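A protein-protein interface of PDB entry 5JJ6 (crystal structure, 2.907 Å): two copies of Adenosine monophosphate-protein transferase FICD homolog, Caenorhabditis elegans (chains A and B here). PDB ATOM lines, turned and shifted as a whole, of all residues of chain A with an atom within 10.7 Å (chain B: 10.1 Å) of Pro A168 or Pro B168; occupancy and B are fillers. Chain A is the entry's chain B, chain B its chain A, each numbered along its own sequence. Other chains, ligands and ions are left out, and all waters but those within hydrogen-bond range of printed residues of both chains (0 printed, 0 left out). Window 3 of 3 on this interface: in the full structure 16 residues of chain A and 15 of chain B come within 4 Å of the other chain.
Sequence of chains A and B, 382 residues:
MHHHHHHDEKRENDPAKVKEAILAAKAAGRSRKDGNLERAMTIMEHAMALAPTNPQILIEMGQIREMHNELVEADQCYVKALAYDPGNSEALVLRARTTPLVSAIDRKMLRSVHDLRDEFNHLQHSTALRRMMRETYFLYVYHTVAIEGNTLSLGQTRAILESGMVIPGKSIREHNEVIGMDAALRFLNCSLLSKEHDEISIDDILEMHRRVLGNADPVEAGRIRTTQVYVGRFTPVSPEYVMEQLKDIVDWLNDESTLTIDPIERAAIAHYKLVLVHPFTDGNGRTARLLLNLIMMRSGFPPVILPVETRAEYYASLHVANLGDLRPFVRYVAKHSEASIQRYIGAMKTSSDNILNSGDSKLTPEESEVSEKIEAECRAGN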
ATOM      1  N   THR A 151     -12.540   4.017  31.747  1.00  0.00           N
ATOM      2  CA  THR A 151     -12.096   5.416  31.788  1.00  0.00           C
ATOM      3  C   THR A 151     -13.030   6.401  31.080  1.00  0.00           C
ATOM      4  O   THR A 151     -12.721   7.581  31.016  1.00  0.00           O
ATOM      5  CB  THR A 151     -10.690   5.583  31.198  1.00  0.00           C
ATOM      6  OG1 THR A 151     -10.753   5.448  29.781  1.00  0.00           O
ATOM      7  CG2 THR A 151      -9.744   4.531  31.747  1.00  0.00           C
ATOM      8  N   LEU A 152     -14.170   5.951  30.568  1.00  0.00           N
ATOM      9  CA  LEU A 152     -15.128   6.902  30.016  1.00  0.00           C
ATOM     10  C   LEU A 152     -15.630   7.860  31.096  1.00  0.00           C
ATOM     11  O   LEU A 152     -15.772   7.498  32.264  1.00  0.00           O
ATOM     12  CB  LEU A 152     -16.302   6.174  29.349  1.00  0.00           C
ATOM     13  CG  LEU A 152     -15.896   5.619  27.963  1.00  0.00           C
ATOM     14  CD1 LEU A 152     -16.935   4.694  27.320  1.00  0.00           C
ATOM     15  CD2 LEU A 152     -15.524   6.761  27.016  1.00  0.00           C
ATOM     16  N   GLN A 156     -19.082  11.615  28.629  1.00  0.00           N
ATOM     17  CA  GLN A 156     -18.894  10.704  27.516  1.00  0.00           C
ATOM     18  C   GLN A 156     -19.919   9.567  27.603  1.00  0.00           C
ATOM     19  O   GLN A 156     -20.472   9.123  26.593  1.00  0.00           O
ATOM     20  CB  GLN A 156     -17.457  10.168  27.515  1.00  0.00           C
ATOM     21  CG  GLN A 156     -16.401  11.234  27.235  1.00  0.00           C
ATOM     22  CD  GLN A 156     -14.968  10.761  27.473  1.00  0.00           C
ATOM     23  OE1 GLN A 156     -14.732   9.832  28.230  1.00  0.00           O
ATOM     24  NE2 GLN A 156     -14.006  11.415  26.827  1.00  0.00           N
ATOM     25  N   ALA A 159     -23.224  10.982  26.612  1.00  0.00           N
ATOM     26  CA  ALA A 159     -23.224  11.189  25.164  1.00  0.00           C
ATOM     27  C   ALA A 159     -23.461   9.887  24.401  1.00  0.00           C
ATOM     28  O   ALA A 159     -24.217   9.858  23.440  1.00  0.00           O
ATOM     29  CB  ALA A 159     -21.929  11.815  24.729  1.00  0.00           C
ATOM     30  N   ILE A 160     -22.797   8.817  24.821  1.00  0.00           N
ATOM     31  CA  ILE A 160     -22.987   7.510  24.206  1.00  0.00           C
ATOM     32  C   ILE A 160     -24.412   6.984  24.388  1.00  0.00           C
ATOM     33  O   ILE A 160     -25.011   6.465  23.461  1.00  0.00           O
ATOM     34  CB  ILE A 160     -22.007   6.481  24.795  1.00  0.00           C
ATOM     35  CG1 ILE A 160     -20.571   6.820  24.408  1.00  0.00           C
ATOM     36  CG2 ILE A 160     -22.344   5.063  24.340  1.00  0.00           C
ATOM     37  CD1 ILE A 160     -19.561   5.910  25.081  1.00  0.00           C
ATOM     38  N   GLY A 164     -26.414   8.754  21.321  1.00  0.00           N
ATOM     39  CA  GLY A 164     -25.975   7.774  20.347  1.00  0.00           C
ATOM     40  C   GLY A 164     -24.666   8.193  19.714  1.00  0.00           C
ATOM     41  O   GLY A 164     -24.332   7.799  18.598  1.00  0.00           O
ATOM     42  N   MET A 165     -23.922   9.006  20.453  1.00  0.00           N
ATOM     43  CA  MET A 165     -22.586   9.422  20.072  1.00  0.00           C
ATOM     44  C   MET A 165     -21.576   8.299  20.281  1.00  0.00           C
ATOM     45  O   MET A 165     -21.907   7.164  20.620  1.00  0.00           O
ATOM     46  CB  MET A 165     -22.121  10.633  20.887  1.00  0.00           C
ATOM     47  CG  MET A 165     -22.857  11.933  20.687  1.00  0.00           C
ATOM     48  SD  MET A 165     -22.793  12.564  19.008  1.00  0.00           S
ATOM     49  CE  MET A 165     -24.534  12.712  18.640  1.00  0.00           C
ATOM     50  N   VAL A 166     -20.330   8.652  20.033  1.00  0.00           N
ATOM     51  CA  VAL A 166     -19.197   7.764  20.086  1.00  0.00           C
ATOM     52  C   VAL A 166     -17.948   8.607  20.376  1.00  0.00           C
ATOM     53  O   VAL A 166     -17.824   9.714  19.846  1.00  0.00           O
ATOM     54  CB  VAL A 166     -19.096   6.978  18.743  1.00  0.00           C
ATOM     55  CG1 VAL A 166     -17.733   7.033  18.144  1.00  0.00           C
ATOM     56  CG2 VAL A 166     -19.650   5.557  18.870  1.00  0.00           C
ATOM     57  N   ILE A 167     -17.062   8.162  21.263  1.00  0.00           N
ATOM     58  CA  ILE A 167     -15.853   8.953  21.481  1.00  0.00           C
ATOM     59  C   ILE A 167     -14.651   8.367  20.727  1.00  0.00           C
ATOM     60  O   ILE A 167     -14.063   7.385  21.165  1.00  0.00           O
ATOM     61  CB  ILE A 167     -15.518   9.088  22.984  1.00  0.00           C
ATOM     62  CG1 ILE A 167     -16.625   9.843  23.706  1.00  0.00           C
ATOM     63  CG2 ILE A 167     -14.270   9.908  23.170  1.00  0.00           C
ATOM     64  CD1 ILE A 167     -17.664   8.974  24.302  1.00  0.00           C
ATOM     65  N   PRO A 168     -14.253   8.988  19.602  1.00  0.00           N
ATOM     66  CA  PRO A 168     -13.125   8.403  18.862  1.00  0.00           C
ATOM     67  C   PRO A 168     -11.774   8.516  19.586  1.00  0.00           C
ATOM     68  O   PRO A 168     -11.564   9.413  20.402  1.00  0.00           O
ATOM     69  CB  PRO A 168     -13.146   9.148  17.523  1.00  0.00           C
ATOM     70  CG  PRO A 168     -13.936  10.316  17.741  1.00  0.00           C
ATOM     71  CD  PRO A 168     -14.924  10.041  18.828  1.00  0.00           C
ATOM     72  N   GLY A 169     -10.887   7.563  19.315  1.00  0.00           N
ATOM     73  CA  GLY A 169      -9.580   7.541  19.945  1.00  0.00           C
ATOM     74  C   GLY A 169      -9.660   6.911  21.320  1.00  0.00           C
ATOM     75  O   GLY A 169      -8.663   6.743  22.029  1.00  0.00           O
ATOM     76  N   LYS A 170     -10.875   6.543  21.693  1.00  0.00           N
ATOM     77  CA  LYS A 170     -11.107   5.891  22.968  1.00  0.00           C
ATOM     78  C   LYS A 170     -11.454   4.406  22.714  1.00  0.00           C
ATOM     79  O   LYS A 170     -11.883   4.032  21.619  1.00  0.00           O
ATOM     80  CB  LYS A 170     -12.189   6.630  23.745  1.00  0.00           C
ATOM     81  CG  LYS A 170     -11.894   6.718  25.213  1.00  0.00           C
ATOM     82  CD  LYS A 170     -12.084   8.103  25.790  1.00  0.00           C
ATOM     83  CE  LYS A 170     -12.041   8.006  27.321  1.00  0.00           C
ATOM     84  NZ  LYS A 170     -10.827   7.330  27.892  1.00  0.00           N
ATOM     85  N   SER A 171     -11.211   3.562  23.706  1.00  0.00           N
ATOM     86  CA  SER A 171     -11.456   2.128  23.585  1.00  0.00           C
ATOM     87  C   SER A 171     -12.873   1.721  23.176  1.00  0.00           C
ATOM     88  O   SER A 171     -13.864   2.130  23.793  1.00  0.00           O
ATOM     89  CB  SER A 171     -11.124   1.497  24.937  1.00  0.00           C
ATOM     90  OG  SER A 171     -11.734   0.235  25.111  1.00  0.00           O
ATOM     91  N   ILE A 172     -12.950   0.862  22.161  1.00  0.00           N
ATOM     92  CA  ILE A 172     -14.217   0.277  21.709  1.00  0.00           C
ATOM     93  C   ILE A 172     -14.859  -0.584  22.797  1.00  0.00           C
ATOM     94  O   ILE A 172     -16.097  -0.616  22.965  1.00  0.00           O
ATOM     95  CB  ILE A 172     -13.995  -0.571  20.440  1.00  0.00           C
ATOM     96  CG1 ILE A 172     -13.349   0.288  19.352  1.00  0.00           C
ATOM     97  CG2 ILE A 172     -15.287  -1.172  19.953  1.00  0.00           C
ATOM     98  CD1 ILE A 172     -12.756  -0.506  18.199  1.00  0.00           C
ATOM     99  N   GLU A 174     -14.680  -0.186  25.987  1.00  0.00           N
ATOM    100  CA  GLU A 174     -15.331   0.649  26.998  1.00  0.00           C
ATOM    101  C   GLU A 174     -16.729   1.112  26.539  1.00  0.00           C
ATOM    102  O   GLU A 174     -17.690   1.119  27.340  1.00  0.00           O
ATOM    103  CB  GLU A 174     -14.466   1.861  27.347  1.00  0.00           C
ATOM    104  CG  GLU A 174     -13.080   1.523  27.856  1.00  0.00           C
ATOM    105  CD  GLU A 174     -12.301   2.760  28.284  1.00  0.00           C
ATOM    106  OE1 GLU A 174     -11.916   3.562  27.382  1.00  0.00           O
ATOM    107  OE2 GLU A 174     -12.053   2.914  29.512  1.00  0.00           O
ATOM    108  N   HIS A 175     -16.834   1.538  25.278  1.00  0.00           N
ATOM    109  CA  HIS A 175     -18.143   1.812  24.693  1.00  0.00           C
ATOM    110  C   HIS A 175     -19.086   0.628  24.890  1.00  0.00           C
ATOM    111  O   HIS A 175     -20.182   0.767  25.459  1.00  0.00           O
ATOM    112  CB  HIS A 175     -18.027   2.129  23.199  1.00  0.00           C
ATOM    113  CG  HIS A 175     -17.383   3.442  22.907  1.00  0.00           C
ATOM    114  ND1 HIS A 175     -16.025   3.656  23.038  1.00  0.00           N
ATOM    115  CD2 HIS A 175     -17.907   4.618  22.494  1.00  0.00           C
ATOM    116  CE1 HIS A 175     -15.744   4.904  22.719  1.00  0.00           C
ATOM    117  NE2 HIS A 175     -16.870   5.513  22.386  1.00  0.00           N
ATOM    118  N   THR B 151     -19.093   1.437   6.071  1.00  0.00           N
ATOM    119  CA  THR B 151     -18.383   2.558   5.443  1.00  0.00           C
ATOM    120  C   THR B 151     -16.926   2.664   5.895  1.00  0.00           C
ATOM    121  O   THR B 151     -16.229   3.614   5.545  1.00  0.00           O
ATOM    122  CB  THR B 151     -19.081   3.919   5.711  1.00  0.00           C
ATOM    123  OG1 THR B 151     -18.823   4.341   7.049  1.00  0.00           O
ATOM    124  CG2 THR B 151     -20.579   3.824   5.501  1.00  0.00           C
ATOM    125  N   LEU B 152     -16.477   1.710   6.700  1.00  0.00           N
ATOM    126  CA  LEU B 152     -15.071   1.647   7.092  1.00  0.00           C
ATOM    127  C   LEU B 152     -14.147   1.364   5.907  1.00  0.00           C
ATOM    128  O   LEU B 152     -14.523   0.665   4.954  1.00  0.00           O
ATOM    129  CB  LEU B 152     -14.879   0.577   8.157  1.00  0.00           C
ATOM    130  CG  LEU B 152     -15.384   0.993   9.540  1.00  0.00           C
ATOM    131  CD1 LEU B 152     -15.389  -0.210  10.471  1.00  0.00           C
ATOM    132  CD2 LEU B 152     -14.518   2.127  10.091  1.00  0.00           C
ATOM    133  N   SER B 153     -12.950   1.942   5.962  1.00  0.00           N
ATOM    134  CA  SER B 153     -11.917   1.702   4.968  1.00  0.00           C
ATOM    135  C   SER B 153     -11.075   0.519   5.411  1.00  0.00           C
ATOM    136  O   SER B 153     -11.174   0.075   6.563  1.00  0.00           O
ATOM    137  CB  SER B 153     -11.042   2.933   4.787  1.00  0.00           C
ATOM    138  OG  SER B 153     -10.046   3.013   5.787  1.00  0.00           O
ATOM    139  N   GLY B 155      -7.828   0.577   5.965  1.00  0.00           N
ATOM    140  CA  GLY B 155      -6.904   1.074   6.970  1.00  0.00           C
ATOM    141  C   GLY B 155      -7.574   1.259   8.308  1.00  0.00           C
ATOM    142  O   GLY B 155      -6.962   1.061   9.358  1.00  0.00           O
ATOM    143  N   GLN B 156      -8.823   1.701   8.266  1.00  0.00           N
ATOM    144  CA  GLN B 156      -9.630   1.841   9.462  1.00  0.00           C
ATOM    145  C   GLN B 156     -10.022   0.468  10.043  1.00  0.00           C
ATOM    146  O   GLN B 156     -10.039   0.286  11.265  1.00  0.00           O
ATOM    147  CB  GLN B 156     -10.864   2.677   9.165  1.00  0.00           C
ATOM    148  CG  GLN B 156     -10.529   4.093   8.817  1.00  0.00           C
ATOM    149  CD  GLN B 156     -11.722   4.840   8.278  1.00  0.00           C
ATOM    150  OE1 GLN B 156     -12.666   4.232   7.796  1.00  0.00           O
ATOM    151  NE2 GLN B 156     -11.675   6.166   8.328  1.00  0.00           N
ATOM    152  N   ALA B 159      -6.962  -0.741  11.658  1.00  0.00           N
ATOM    153  CA  ALA B 159      -6.761   0.037  12.882  1.00  0.00           C
ATOM    154  C   ALA B 159      -7.640  -0.506  14.003  1.00  0.00           C
ATOM    155  O   ALA B 159      -7.193  -0.638  15.142  1.00  0.00           O
ATOM    156  CB  ALA B 159      -7.061   1.500  12.652  1.00  0.00           C
ATOM    157  N   ILE B 160      -8.891  -0.823  13.678  1.00  0.00           N
ATOM    158  CA  ILE B 160      -9.795  -1.360  14.672  1.00  0.00           C
ATOM    159  C   ILE B 160      -9.257  -2.684  15.223  1.00  0.00           C
ATOM    160  O   ILE B 160      -9.198  -2.877  16.446  1.00  0.00           O
ATOM    161  CB  ILE B 160     -11.202  -1.546  14.113  1.00  0.00           C
ATOM    162  CG1 ILE B 160     -11.845  -0.184  13.870  1.00  0.00           C
ATOM    163  CG2 ILE B 160     -12.061  -2.328  15.098  1.00  0.00           C
ATOM    164  CD1 ILE B 160     -13.208  -0.260  13.247  1.00  0.00           C
ATOM    165  N   GLY B 164      -7.843  -1.286  18.496  1.00  0.00           N
ATOM    166  CA  GLY B 164      -9.110  -1.303  19.193  1.00  0.00           C
ATOM    167  C   GLY B 164      -9.595   0.046  19.665  1.00  0.00           C
ATOM    168  O   GLY B 164     -10.428   0.105  20.558  1.00  0.00           O
ATOM    169  N   MET B 165      -9.058   1.137  19.121  1.00  0.00           N
ATOM    170  CA  MET B 165      -9.621   2.449  19.430  1.00  0.00           C
ATOM    171  C   MET B 165     -10.763   2.778  18.464  1.00  0.00           C
ATOM    172  O   MET B 165     -10.957   2.099  17.462  1.00  0.00           O
ATOM    173  CB  MET B 165      -8.543   3.526  19.398  1.00  0.00           C
ATOM    174  CG  MET B 165      -7.472   3.308  20.438  1.00  0.00           C
ATOM    175  SD  MET B 165      -8.166   3.238  22.106  1.00  0.00           S
ATOM    176  CE  MET B 165      -7.644   1.611  22.637  1.00  0.00           C
ATOM    177  N   VAL B 166     -11.455   3.880  18.703  1.00  0.00           N
ATOM    178  CA  VAL B 166     -12.630   4.195  17.910  1.00  0.00           C
ATOM    179  C   VAL B 166     -12.242   5.134  16.765  1.00  0.00           C
ATOM    180  O   VAL B 166     -11.479   6.085  16.965  1.00  0.00           O
ATOM    181  CB  VAL B 166     -13.729   4.833  18.784  1.00  0.00           C
ATOM    182  CG1 VAL B 166     -14.729   5.552  17.918  1.00  0.00           C
ATOM    183  CG2 VAL B 166     -14.478   3.745  19.558  1.00  0.00           C
ATOM    184  N   ILE B 167     -12.793   4.874  15.581  1.00  0.00           N
ATOM    185  CA  ILE B 167     -12.506   5.638  14.377  1.00  0.00           C
ATOM    186  C   ILE B 167     -13.487   6.808  14.257  1.00  0.00           C
ATOM    187  O   ILE B 167     -14.692   6.624  14.422  1.00  0.00           O
ATOM    188  CB  ILE B 167     -12.621   4.753  13.107  1.00  0.00           C
ATOM    189  CG1 ILE B 167     -11.799   3.463  13.231  1.00  0.00           C
ATOM    190  CG2 ILE B 167     -12.272   5.547  11.854  1.00  0.00           C
ATOM    191  CD1 ILE B 167     -10.343   3.669  13.482  1.00  0.00           C
ATOM    192  N   PRO B 168     -12.979   8.029  14.015  1.00  0.00           N
ATOM    193  CA  PRO B 168     -13.919   9.160  13.940  1.00  0.00           C
ATOM    194  C   PRO B 168     -14.917   9.041  12.801  1.00  0.00           C
ATOM    195  O   PRO B 168     -14.596   8.498  11.747  1.00  0.00           O
ATOM    196  CB  PRO B 168     -13.005  10.373  13.710  1.00  0.00           C
ATOM    197  CG  PRO B 168     -11.725   9.820  13.244  1.00  0.00           C
ATOM    198  CD  PRO B 168     -11.584   8.451  13.828  1.00  0.00           C
ATOM    199  N   GLY B 169     -16.130   9.524  13.038  1.00  0.00           N
ATOM    200  CA  GLY B 169     -17.171   9.483  12.034  1.00  0.00           C
ATOM    201  C   GLY B 169     -17.886   8.158  11.827  1.00  0.00           C
ATOM    202  O   GLY B 169     -18.792   8.097  11.010  1.00  0.00           O
ATOM    203  N   LYS B 170     -17.499   7.096  12.526  1.00  0.00           N
ATOM    204  CA  LYS B 170     -18.200   5.822  12.338  1.00  0.00           C
ATOM    205  C   LYS B 170     -19.050   5.372  13.536  1.00  0.00           C
ATOM    206  O   LYS B 170     -18.672   5.562  14.689  1.00  0.00           O
ATOM    207  CB  LYS B 170     -17.184   4.733  12.014  1.00  0.00           C
ATOM    208  CG  LYS B 170     -16.221   5.109  10.919  1.00  0.00           C
ATOM    209  CD  LYS B 170     -16.953   5.371   9.622  1.00  0.00           C
ATOM    210  CE  LYS B 170     -15.982   5.763   8.519  1.00  0.00           C
ATOM    211  NZ  LYS B 170     -16.717   6.287   7.346  1.00  0.00           N
ATOM    212  N   SER B 171     -20.194   4.762  13.231  1.00  0.00           N
ATOM    213  CA  SER B 171     -21.126   4.215  14.216  1.00  0.00           C
ATOM    214  C   SER B 171     -20.481   3.077  15.000  1.00  0.00           C
ATOM    215  O   SER B 171     -19.659   2.341  14.444  1.00  0.00           O
ATOM    216  CB  SER B 171     -22.416   3.736  13.548  1.00  0.00           C
ATOM    217  OG  SER B 171     -22.249   2.459  12.953  1.00  0.00           O
ATOM    218  N   ILE B 172     -20.843   2.929  16.277  1.00  0.00           N
ATOM    219  CA  ILE B 172     -20.378   1.791  17.077  1.00  0.00           C
ATOM    220  C   ILE B 172     -20.754   0.460  16.400  1.00  0.00           C
ATOM    221  O   ILE B 172     -20.009  -0.518  16.483  1.00  0.00           O
ATOM    222  CB  ILE B 172     -20.945   1.833  18.520  1.00  0.00           C
ATOM    223  CG1 ILE B 172     -20.115   0.967  19.462  1.00  0.00           C
ATOM    224  CG2 ILE B 172     -22.382   1.369  18.563  1.00  0.00           C
ATOM    225  CD1 ILE B 172     -18.694   1.450  19.617  1.00  0.00           C
ATOM    226  N   GLU B 174     -20.705  -0.331  13.211  1.00  0.00           N
ATOM    227  CA  GLU B 174     -19.718  -0.691  12.182  1.00  0.00           C
ATOM    228  C   GLU B 174     -18.445  -1.306  12.783  1.00  0.00           C
ATOM    229  O   GLU B 174     -17.957  -2.375  12.328  1.00  0.00           O
ATOM    230  CB  GLU B 174     -19.369   0.540  11.330  1.00  0.00           C
ATOM    231  CG  GLU B 174     -20.557   1.169  10.596  1.00  0.00           C
ATOM    232  CD  GLU B 174     -20.167   2.360   9.695  1.00  0.00           C
ATOM    233  OE1 GLU B 174     -19.854   3.454  10.235  1.00  0.00           O
ATOM    234  OE2 GLU B 174     -20.165   2.203   8.448  1.00  0.00           O
ATOM    235  N   HIS B 175     -17.931  -0.648  13.818  1.00  0.00           N
ATOM    236  CA  HIS B 175     -16.822  -1.183  14.598  1.00  0.00           C
ATOM    237  C   HIS B 175     -17.149  -2.605  15.017  1.00  0.00           C
ATOM    238  O   HIS B 175     -16.343  -3.530  14.856  1.00  0.00           O
ATOM    239  CB  HIS B 175     -16.556  -0.367  15.858  1.00  0.00           C
ATOM    240  CG  HIS B 175     -16.103   1.039  15.604  1.00  0.00           C
ATOM    241  ND1 HIS B 175     -16.965   2.036  15.216  1.00  0.00           N
ATOM    242  CD2 HIS B 175     -14.883   1.613  15.718  1.00  0.00           C
ATOM    243  CE1 HIS B 175     -16.299   3.174  15.103  1.00  0.00           C
ATOM    244  NE2 HIS B 175     -15.037   2.941  15.396  1.00  0.00           N
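Printed residues of chain B that touch a printed residue of chain A: Ile B160, Gly B164, Met B165, Val B166, Pro B168, Lys B170, Ile B172 and His B175. Hydrophobic or aromatic side chains of chain B within 4 Å of the printed part of chain A: Ile B160, Met B165, Val B166, Ile B172 and His B175. Along chain B the printed residues that touch a printed residue of chain A span positions 160 to 175. Printed residues of chain A that touch a printed residue of chain B: Val A166, Ile A167, Pro A168, Gly A169, Lys A170, Ser A171, Ile A172 and His A175. Hydrophobic or aromatic side chains of chain A within 4 Å of the printed part of chain B: Val A166, Pro A168, Ile A172 and His A175.
Val B166 touches its own counterpart, Val A166. Lys A170 touches Met B165, but with the chains exchanged Met A165 does not touch Lys B170 (6.9 Å). Ile A172 touches Ile B160, but with the chains exchanged Ile A160 does not touch Ile B172 (6.7 Å). His A175 touches Val B166, but with the chains exchanged Val A166 does not touch His B175 (5.1 Å). Positions printed for both chains: 151, 152, 156, 159, 160, 164, 165, 166, 167, 168, 169, 170, 171, 172, 174 and 175. Of the 19 pairs that touch across the chains among the printed residues, 8 have their exchanged pair printed and touching as well.
Among the printed residues, pairs that only touch across the chains: Val A166 with Val B166 (3.4 Å), Val A166 with Lys B170 (3.9 Å), Val A166 with Ile B172 (3.9 Å), Ile A167 with Val B166 (3.5 Å), Pro A168 with Val B166 (3.4 Å), Pro A168 with Pro B168 (3.7 Å), Lys A170 with Met B165 (3.5 Å), Ser A171 with Gly B164 (3.8 Å), Ile A172 with Ile B160 (3.7 Å), Ile A172 with Met B165 (3.3 Å), Ile A172 with Val B166 (3.6 Å), Ile A172 with His B175 (3.9 Å), His A175 with Val B166 (3.6 Å) and His A175 with Ile B172 (3.7 Å).
The backbone carbonyl oxygen (O) of Lys A170 is in hydrogen-bond range of the backbone NH (N) of Val B166 (3.0 Å). The side-chain sulfur (SD) of Met B165 sits at hydrogen-bond distance from the backbone NH (N) of Ser A171 (3.5 Å). The backbone carbonyl oxygen (O) of Gly B164 is in hydrogen-bond range of the backbone NH (N) of Ile A172, 3.1 Å away. N of Gly A169 lies within hydrogen-bond range of O of Val B166. O of Gly A169 lies close to SD of Met B165, at 3.5 Å.
OG1 of Thr A151 is in hydrogen-bond range of NZ of Lys A170 (2.7 Å). The side-chain amino group (NZ) of Lys A170 is in salt-bridge range of the side-chain carboxylate (OE1) of Glu A174. A ring nitrogen (ND1) of His A175 sits at hydrogen-bond distance from the backbone carbonyl oxygen (O) of Ser A171. The backbone carbonyl oxygen of Ala B159 lies within hydrogen-bond range of the backbone NH of Gly B164 (3.5 Å). N of Glu A174 lies within hydrogen-bond range of OG of Ser A171 (3.1 Å). N of Ile B167 lies within hydrogen-bond range of NE2 of His B175 (3.0 Å).
Pro A168 touches just these residues of chain B: Val B166 and Pro B168. Pro B168 touches just one residue of chain A: Pro A168 (3.7 Å). Of chain B, only Val B166 comes within 4 Å of Ile A167. Gly A169 touches just these residues of chain B: Met B165 (3.5 Å) and Val B166 (2.8 Å). Val B166 touches just these residues of chain A: Val A166, Ile A167, Pro A168, Gly A169, Lys A170, Ile A172 and His A175. No residue of chain A comes within 4 Å of Ile B167. No residue of chain A comes within 4 Å of Gly B169. Lys B170 touches one residue of chain A. Of the printed residues of chain A, Ile B172 touches Val A166 (3.9 Å) and His A175 (3.7 Å). Of the printed residues of chain A, Ile B160 touches Ile A172. Of the printed residues of chain A, Met B165 touches Gly A169 (3.5 Å), Lys A170 (3.5 Å), Ser A171 (3.5 Å) and Ile A172 (3.3 Å). Printed residues of chain A within 4 Å of His B175: Ile A172 (3.9 Å). Of the printed residues of chain A, Gly B164 touches Ser A171 (3.8 Å) and Ile A172 (3.1 Å). Thr B151 touches none of the printed residues of chain A. Glu B174 touches none of the printed residues of chain A.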
